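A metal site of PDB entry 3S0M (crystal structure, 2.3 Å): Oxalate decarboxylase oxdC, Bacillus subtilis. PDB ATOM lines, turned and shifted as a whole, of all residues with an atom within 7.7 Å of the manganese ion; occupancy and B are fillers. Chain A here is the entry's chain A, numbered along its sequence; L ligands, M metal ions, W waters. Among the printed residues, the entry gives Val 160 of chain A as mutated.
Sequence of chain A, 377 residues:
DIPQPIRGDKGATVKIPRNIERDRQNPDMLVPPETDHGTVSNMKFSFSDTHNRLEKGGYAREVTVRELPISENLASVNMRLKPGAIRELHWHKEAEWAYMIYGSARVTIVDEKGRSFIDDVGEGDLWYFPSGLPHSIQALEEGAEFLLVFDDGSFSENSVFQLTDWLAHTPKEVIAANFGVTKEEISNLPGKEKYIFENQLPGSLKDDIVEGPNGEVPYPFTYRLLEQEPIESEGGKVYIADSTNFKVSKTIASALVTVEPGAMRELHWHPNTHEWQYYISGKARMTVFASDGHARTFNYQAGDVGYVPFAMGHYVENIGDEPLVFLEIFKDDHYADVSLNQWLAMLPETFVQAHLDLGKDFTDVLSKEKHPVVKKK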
ATOM      1  N   MET A  79      31.875   2.285  -9.512  1.00  0.00           N
ATOM      2  CA  MET A  79      32.086   2.707 -10.899  1.00  0.00           C
ATOM      3  C   MET A  79      31.827   4.195 -11.120  1.00  0.00           C
ATOM      4  O   MET A  79      30.984   4.799 -10.452  1.00  0.00           O
ATOM      5  CB  MET A  79      31.217   1.879 -11.847  1.00  0.00           C
ATOM      6  CG  MET A  79      31.408   2.205 -13.307  1.00  0.00           C
ATOM      7  SD  MET A  79      30.580   1.035 -14.398  1.00  0.00           S
ATOM      8  CE  MET A  79      31.617  -0.425 -14.211  1.00  0.00           C
ATOM      9  N   ARG A  87      29.097   2.755 -20.250  1.00  0.00           N
ATOM     10  CA  ARG A  87      29.530   1.437 -19.822  1.00  0.00           C
ATOM     11  C   ARG A  87      28.945   0.452 -20.818  1.00  0.00           C
ATOM     12  O   ARG A  87      27.744   0.220 -20.823  1.00  0.00           O
ATOM     13  CB  ARG A  87      28.987   1.142 -18.420  1.00  0.00           C
ATOM     14  CG  ARG A  87      29.229  -0.284 -17.978  1.00  0.00           C
ATOM     15  CD  ARG A  87      30.700  -0.663 -18.061  1.00  0.00           C
ATOM     16  NE  ARG A  87      30.928  -2.012 -17.572  1.00  0.00           N
ATOM     17  CZ  ARG A  87      31.026  -3.086 -18.358  1.00  0.00           C
ATOM     18  NH1 ARG A  87      30.929  -2.969 -19.673  1.00  0.00           N
ATOM     19  NH2 ARG A  87      31.219  -4.281 -17.807  1.00  0.00           N
ATOM     20  N   GLU A  88      29.800  -0.110 -21.670  1.00  0.00           N
ATOM     21  CA  GLU A  88      29.378  -0.925 -22.819  1.00  0.00           C
ATOM     22  C   GLU A  88      28.272  -1.940 -22.558  1.00  0.00           C
ATOM     23  O   GLU A  88      28.221  -2.595 -21.521  1.00  0.00           O
ATOM     24  CB  GLU A  88      30.576  -1.651 -23.430  1.00  0.00           C
ATOM     25  CG  GLU A  88      30.245  -2.391 -24.721  1.00  0.00           C
ATOM     26  CD  GLU A  88      31.409  -3.173 -25.269  1.00  0.00           C
ATOM     27  OE1 GLU A  88      32.564  -2.914 -24.881  1.00  0.00           O
ATOM     28  OE2 GLU A  88      31.157  -4.071 -26.111  1.00  0.00           O
ATOM     29  N   HIS A  90      26.348  -5.049 -22.108  1.00  0.00           N
ATOM     30  CA  HIS A  90      26.930  -6.279 -21.572  1.00  0.00           C
ATOM     31  C   HIS A  90      25.925  -7.097 -20.775  1.00  0.00           C
ATOM     32  O   HIS A  90      24.819  -6.649 -20.489  1.00  0.00           O
ATOM     33  CB  HIS A  90      28.131  -5.948 -20.678  1.00  0.00           C
ATOM     34  CG  HIS A  90      27.763  -5.331 -19.362  1.00  0.00           C
ATOM     35  ND1 HIS A  90      27.652  -3.967 -19.188  1.00  0.00           N
ATOM     36  CD2 HIS A  90      27.482  -5.882 -18.153  1.00  0.00           C
ATOM     37  CE1 HIS A  90      27.322  -3.705 -17.926  1.00  0.00           C
ATOM     38  NE2 HIS A  90      27.216  -4.847 -17.291  1.00  0.00           N
ATOM     39  N   TRP A  91      26.325  -8.303 -20.408  1.00  0.00           N
ATOM     40  CA  TRP A  91      25.534  -9.095 -19.490  1.00  0.00           C
ATOM     41  C   TRP A  91      26.440  -9.953 -18.626  1.00  0.00           C
ATOM     42  O   TRP A  91      27.656  -9.998 -18.830  1.00  0.00           O
ATOM     43  CB  TRP A  91      24.519  -9.953 -20.249  1.00  0.00           C
ATOM     44  CG  TRP A  91      25.084 -11.112 -21.021  1.00  0.00           C
ATOM     45  CD1 TRP A  91      25.083 -12.421 -20.634  1.00  0.00           C
ATOM     46  CD2 TRP A  91      25.716 -11.074 -22.311  1.00  0.00           C
ATOM     47  NE1 TRP A  91      25.677 -13.203 -21.603  1.00  0.00           N
ATOM     48  CE2 TRP A  91      26.073 -12.409 -22.642  1.00  0.00           C
ATOM     49  CE3 TRP A  91      26.006 -10.055 -23.219  1.00  0.00           C
ATOM     50  CZ2 TRP A  91      26.704 -12.731 -23.847  1.00  0.00           C
ATOM     51  CZ3 TRP A  91      26.634 -10.386 -24.421  1.00  0.00           C
ATOM     52  CH2 TRP A  91      26.978 -11.714 -24.712  1.00  0.00           C
ATOM     53  N   HIS A  92      25.856 -10.624 -17.643  1.00  0.00           N
ATOM     54  CA  HIS A  92      26.618 -11.558 -16.817  1.00  0.00           C
ATOM     55  C   HIS A  92      25.724 -12.541 -16.035  1.00  0.00           C
ATOM     56  O   HIS A  92      24.493 -12.369 -15.929  1.00  0.00           O
ATOM     57  CB  HIS A  92      27.555 -10.789 -15.879  1.00  0.00           C
ATOM     58  CG  HIS A  92      26.963  -9.504 -15.375  1.00  0.00           C
ATOM     59  ND1 HIS A  92      25.808  -9.470 -14.636  1.00  0.00           N
ATOM     60  CD2 HIS A  92      27.375  -8.231 -15.501  1.00  0.00           C
ATOM     61  CE1 HIS A  92      25.515  -8.209 -14.331  1.00  0.00           C
ATOM     62  NE2 HIS A  92      26.453  -7.441 -14.857  1.00  0.00           N
ATOM     63  N   GLU A  94      25.629 -13.043 -12.857  1.00  0.00           N
ATOM     64  CA  GLU A  94      25.161 -12.503 -11.600  1.00  0.00           C
ATOM     65  C   GLU A  94      24.031 -11.507 -11.805  1.00  0.00           C
ATOM     66  O   GLU A  94      24.007 -10.808 -12.816  1.00  0.00           O
ATOM     67  CB  GLU A  94      26.312 -11.831 -10.859  1.00  0.00           C
ATOM     68  CG  GLU A  94      27.492 -12.776 -10.587  1.00  0.00           C
ATOM     69  CD  GLU A  94      28.464 -12.888 -11.756  1.00  0.00           C
ATOM     70  OE1 GLU A  94      28.157 -12.408 -12.873  1.00  0.00           O
ATOM     71  OE2 GLU A  94      29.561 -13.465 -11.561  1.00  0.00           O
ATOM     72  N   ALA A  95      23.099 -11.456 -10.868  1.00  0.00           N
ATOM     73  CA  ALA A  95      22.127 -10.365 -10.840  1.00  0.00           C
ATOM     74  C   ALA A  95      22.839  -9.124 -10.294  1.00  0.00           C
ATOM     75  O   ALA A  95      23.802  -9.227  -9.537  1.00  0.00           O
ATOM     76  CB  ALA A  95      20.934 -10.732  -9.982  1.00  0.00           C
ATOM     77  N   GLU A  96      22.362  -7.945 -10.684  1.00  0.00           N
ATOM     78  CA  GLU A  96      23.030  -6.705 -10.308  1.00  0.00           C
ATOM     79  C   GLU A  96      22.108  -5.691  -9.627  1.00  0.00           C
ATOM     80  O   GLU A  96      21.017  -5.415 -10.107  1.00  0.00           O
ATOM     81  CB  GLU A  96      23.690  -6.091 -11.546  1.00  0.00           C
ATOM     82  CG  GLU A  96      24.148  -4.664 -11.409  1.00  0.00           C
ATOM     83  CD  GLU A  96      24.727  -4.139 -12.722  1.00  0.00           C
ATOM     84  OE1 GLU A  96      25.150  -4.979 -13.545  1.00  0.00           O
ATOM     85  OE2 GLU A  96      24.725  -2.912 -12.933  1.00  0.00           O
ATOM     86  N   TRP A 127      18.749   0.639  -9.331  1.00  0.00           N
ATOM     87  CA  TRP A 127      18.257  -0.232 -10.387  1.00  0.00           C
ATOM     88  C   TRP A 127      18.575  -1.677 -10.022  1.00  0.00           C
ATOM     89  O   TRP A 127      19.372  -1.929  -9.118  1.00  0.00           O
ATOM     90  CB  TRP A 127      18.804   0.157 -11.770  1.00  0.00           C
ATOM     91  CG  TRP A 127      20.259  -0.130 -12.023  1.00  0.00           C
ATOM     92  CD1 TRP A 127      20.860  -1.359 -12.102  1.00  0.00           C
ATOM     93  CD2 TRP A 127      21.287   0.833 -12.288  1.00  0.00           C
ATOM     94  NE1 TRP A 127      22.203  -1.215 -12.372  1.00  0.00           N
ATOM     95  CE2 TRP A 127      22.487   0.126 -12.492  1.00  0.00           C
ATOM     96  CE3 TRP A 127      21.307   2.228 -12.345  1.00  0.00           C
ATOM     97  CZ2 TRP A 127      23.679   0.757 -12.754  1.00  0.00           C
ATOM     98  CZ3 TRP A 127      22.486   2.849 -12.615  1.00  0.00           C
ATOM     99  CH2 TRP A 127      23.658   2.115 -12.831  1.00  0.00           C
ATOM    100  N   PHE A 129      19.092  -5.410 -12.230  1.00  0.00           N
ATOM    101  CA  PHE A 129      19.027  -6.212 -13.443  1.00  0.00           C
ATOM    102  C   PHE A 129      19.142  -7.671 -13.086  1.00  0.00           C
ATOM    103  O   PHE A 129      20.175  -8.091 -12.566  1.00  0.00           O
ATOM    104  CB  PHE A 129      20.160  -5.831 -14.382  1.00  0.00           C
ATOM    105  CG  PHE A 129      20.227  -4.371 -14.684  1.00  0.00           C
ATOM    106  CD1 PHE A 129      21.450  -3.746 -14.870  1.00  0.00           C
ATOM    107  CD2 PHE A 129      19.079  -3.610 -14.785  1.00  0.00           C
ATOM    108  CE1 PHE A 129      21.526  -2.393 -15.156  1.00  0.00           C
ATOM    109  CE2 PHE A 129      19.132  -2.260 -15.070  1.00  0.00           C
ATOM    110  CZ  PHE A 129      20.362  -1.651 -15.261  1.00  0.00           C
ATOM    111  N   LEU A 133      20.290 -10.776 -17.980  1.00  0.00           N
ATOM    112  CA  LEU A 133      19.671  -9.825 -18.906  1.00  0.00           C
ATOM    113  C   LEU A 133      20.668  -8.731 -19.302  1.00  0.00           C
ATOM    114  O   LEU A 133      21.344  -8.169 -18.443  1.00  0.00           O
ATOM    115  CB  LEU A 133      18.420  -9.205 -18.301  1.00  0.00           C
ATOM    116  CG  LEU A 133      17.318 -10.156 -17.818  1.00  0.00           C
ATOM    117  CD1 LEU A 133      16.197  -9.343 -17.205  1.00  0.00           C
ATOM    118  CD2 LEU A 133      16.779 -11.032 -18.936  1.00  0.00           C
ATOM    119  N   PRO A 134      20.771  -8.464 -20.604  1.00  0.00           N
ATOM    120  CA  PRO A 134      21.728  -7.497 -21.147  1.00  0.00           C
ATOM    121  C   PRO A 134      21.362  -6.070 -20.785  1.00  0.00           C
ATOM    122  O   PRO A 134      20.183  -5.706 -20.810  1.00  0.00           O
ATOM    123  CB  PRO A 134      21.622  -7.703 -22.666  1.00  0.00           C
ATOM    124  CG  PRO A 134      20.220  -8.160 -22.870  1.00  0.00           C
ATOM    125  CD  PRO A 134      19.926  -9.043 -21.671  1.00  0.00           C
ATOM    126  N   HIS A 135      22.368  -5.269 -20.452  1.00  0.00           N
ATOM    127  CA  HIS A 135      22.117  -3.893 -20.028  1.00  0.00           C
ATOM    128  C   HIS A 135      23.253  -2.949 -20.370  1.00  0.00           C
ATOM    129  O   HIS A 135      24.260  -3.361 -20.966  1.00  0.00           O
ATOM    130  CB  HIS A 135      21.821  -3.845 -18.521  1.00  0.00           C
ATOM    131  CG  HIS A 135      22.811  -4.609 -17.689  1.00  0.00           C
ATOM    132  ND1 HIS A 135      22.676  -5.960 -17.426  1.00  0.00           N
ATOM    133  CD2 HIS A 135      23.936  -4.209 -17.054  1.00  0.00           C
ATOM    134  CE1 HIS A 135      23.678  -6.355 -16.671  1.00  0.00           C
ATOM    135  NE2 HIS A 135      24.462  -5.310 -16.426  1.00  0.00           N
ATOM    136  N   SER A 136      23.087  -1.696 -19.997  1.00  0.00           N
ATOM    137  CA  SER A 136      24.117  -0.678 -20.229  1.00  0.00           C
ATOM    138  C   SER A 136      23.816   0.548 -19.392  1.00  0.00           C
ATOM    139  O   SER A 136      22.661   0.796 -19.026  1.00  0.00           O
ATOM    140  CB  SER A 136      24.164  -0.273 -21.697  1.00  0.00           C
ATOM    141  OG  SER A 136      22.965   0.390 -22.061  1.00  0.00           O
ATOM    142  N   ILE A 137      24.844   1.329 -19.126  1.00  0.00           N
ATOM    143  CA  ILE A 137      24.689   2.579 -18.402  1.00  0.00           C
ATOM    144  C   ILE A 137      25.309   3.688 -19.211  1.00  0.00           C
ATOM    145  O   ILE A 137      26.359   3.497 -19.800  1.00  0.00           O
ATOM    146  CB  ILE A 137      25.408   2.521 -17.048  1.00  0.00           C
ATOM    147  CG1 ILE A 137      25.086   1.212 -16.335  1.00  0.00           C
ATOM    148  CG2 ILE A 137      25.022   3.713 -16.201  1.00  0.00           C
ATOM    149  CD1 ILE A 137      26.071   0.845 -15.262  1.00  0.00           C
ATOM    150  N   LEU A 148      27.779  -0.796  -7.441  1.00  0.00           N
ATOM    151  CA  LEU A 148      27.104  -1.975  -7.966  1.00  0.00           C
ATOM    152  C   LEU A 148      27.278  -3.141  -7.001  1.00  0.00           C
ATOM    153  O   LEU A 148      28.354  -3.330  -6.445  1.00  0.00           O
ATOM    154  CB  LEU A 148      27.667  -2.343  -9.336  1.00  0.00           C
ATOM    155  CG  LEU A 148      27.671  -1.196 -10.345  1.00  0.00           C
ATOM    156  CD1 LEU A 148      28.255  -1.655 -11.672  1.00  0.00           C
ATOM    157  CD2 LEU A 148      26.267  -0.650 -10.511  1.00  0.00           C
ATOM    158  N   PHE A 150      26.714  -7.416  -6.771  1.00  0.00           N
ATOM    159  CA  PHE A 150      26.442  -8.635  -7.532  1.00  0.00           C
ATOM    160  C   PHE A 150      26.268  -9.813  -6.588  1.00  0.00           C
ATOM    161  O   PHE A 150      27.022  -9.940  -5.622  1.00  0.00           O
ATOM    162  CB  PHE A 150      27.545  -8.881  -8.546  1.00  0.00           C
ATOM    163  CG  PHE A 150      27.758  -7.747  -9.485  1.00  0.00           C
ATOM    164  CD1 PHE A 150      27.150  -7.732 -10.727  1.00  0.00           C
ATOM    165  CD2 PHE A 150      28.556  -6.677  -9.122  1.00  0.00           C
ATOM    166  CE1 PHE A 150      27.350  -6.684 -11.604  1.00  0.00           C
ATOM    167  CE2 PHE A 150      28.750  -5.613  -9.994  1.00  0.00           C
ATOM    168  CZ  PHE A 150      28.146  -5.623 -11.238  1.00  0.00           C
ATOM    169  N   PHE A 155      32.419 -12.818  -8.396  1.00  0.00           N
ATOM    170  CA  PHE A 155      32.325 -11.861  -9.499  1.00  0.00           C
ATOM    171  C   PHE A 155      33.618 -11.049  -9.718  1.00  0.00           C
ATOM    172  O   PHE A 155      34.321 -10.676  -8.770  1.00  0.00           O
ATOM    173  CB  PHE A 155      31.128 -10.927  -9.279  1.00  0.00           C
ATOM    174  CG  PHE A 155      30.983  -9.830 -10.315  1.00  0.00           C
ATOM    175  CD1 PHE A 155      30.119  -9.983 -11.395  1.00  0.00           C
ATOM    176  CD2 PHE A 155      31.696  -8.655 -10.213  1.00  0.00           C
ATOM    177  CE1 PHE A 155      29.991  -8.973 -12.347  1.00  0.00           C
ATOM    178  CE2 PHE A 155      31.578  -7.644 -11.154  1.00  0.00           C
ATOM    179  CZ  PHE A 155      30.723  -7.798 -12.223  1.00  0.00           C
ATOM    180  N   VAL A 160      33.161  -9.948 -17.408  1.00  0.00           N
ATOM    181  CA  VAL A 160      31.771  -9.752 -17.768  1.00  0.00           C
ATOM    182  C   VAL A 160      31.657 -10.048 -19.266  1.00  0.00           C
ATOM    183  O   VAL A 160      32.676 -10.092 -19.939  1.00  0.00           O
ATOM    184  CB  VAL A 160      31.355  -8.327 -17.427  1.00  0.00           C
ATOM    185  CG1 VAL A 160      30.086  -7.930 -18.144  1.00  0.00           C
ATOM    186  CG2 VAL A 160      31.190  -8.189 -15.919  1.00  0.00           C
ATOM    187  N   GLN A 162      30.881  -8.688 -22.703  1.00  0.00           N
ATOM    188  CA  GLN A 162      30.715  -7.465 -23.497  1.00  0.00           C
ATOM    189  C   GLN A 162      30.237  -7.759 -24.926  1.00  0.00           C
ATOM    190  O   GLN A 162      30.677  -8.720 -25.568  1.00  0.00           O
ATOM    191  CB  GLN A 162      32.042  -6.690 -23.565  1.00  0.00           C
ATOM    192  CG  GLN A 162      32.210  -5.572 -22.526  1.00  0.00           C
ATOM    193  CD  GLN A 162      32.406  -6.102 -21.117  1.00  0.00           C
ATOM    194  OE1 GLN A 162      33.446  -6.685 -20.804  1.00  0.00           O
ATOM    195  NE2 GLN A 162      31.421  -5.906 -20.264  1.00  0.00           N
HETATM  196  O1  LIG L   1      31.024  -4.289 -14.773  1.00  0.00           O
HETATM  197  O2  LIG L   1      28.846  -4.814 -14.517  1.00  0.00           O
HETATM  198  O3  LIG L   1      29.515  -2.617 -14.871  1.00  0.00           O
HETATM  199 MN    MN M   1      26.482  -5.019 -15.276  1.00  0.00          MN
HETATM  200  O   HOH W   1      25.971  -2.656 -15.077  1.00  0.00           O
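The backbone carbonyl oxygen of Glu 88 sits at hydrogen-bond distance from a ring nitrogen (ND1) of His 90, at 2.8 Å.
The backbone carbonyl oxygen of Glu 96 lies within hydrogen-bond range of the backbone NH of Phe 129, at 2.9 Å.
A ring nitrogen (ND1) of His 135 lies within hydrogen-bond range of the backbone carbonyl oxygen (O) of Leu 133, at 2.8 Å.
A ring nitrogen (ND1) of His 92 is in hydrogen-bond range of the backbone carbonyl oxygen of Glu 94 (2.9 Å).
The indole nitrogen of Trp 127 lies within hydrogen-bond range of the side-chain carboxylate of Glu 96, at 3.1 Å.
ND1 of His 90 lies within hydrogen-bond range of NH1 of Arg 87, 3.5 Å away.
The manganese ion is bound by NE2 of His 90 (2.2 Å), OE1 of Glu 96 (2.2 Å), NE2 of His 135 (2.3 Å), water W1 (2.4 Å), NE2 of His 92 (2.5 Å) and O2 of the ligand (2.5 Å).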
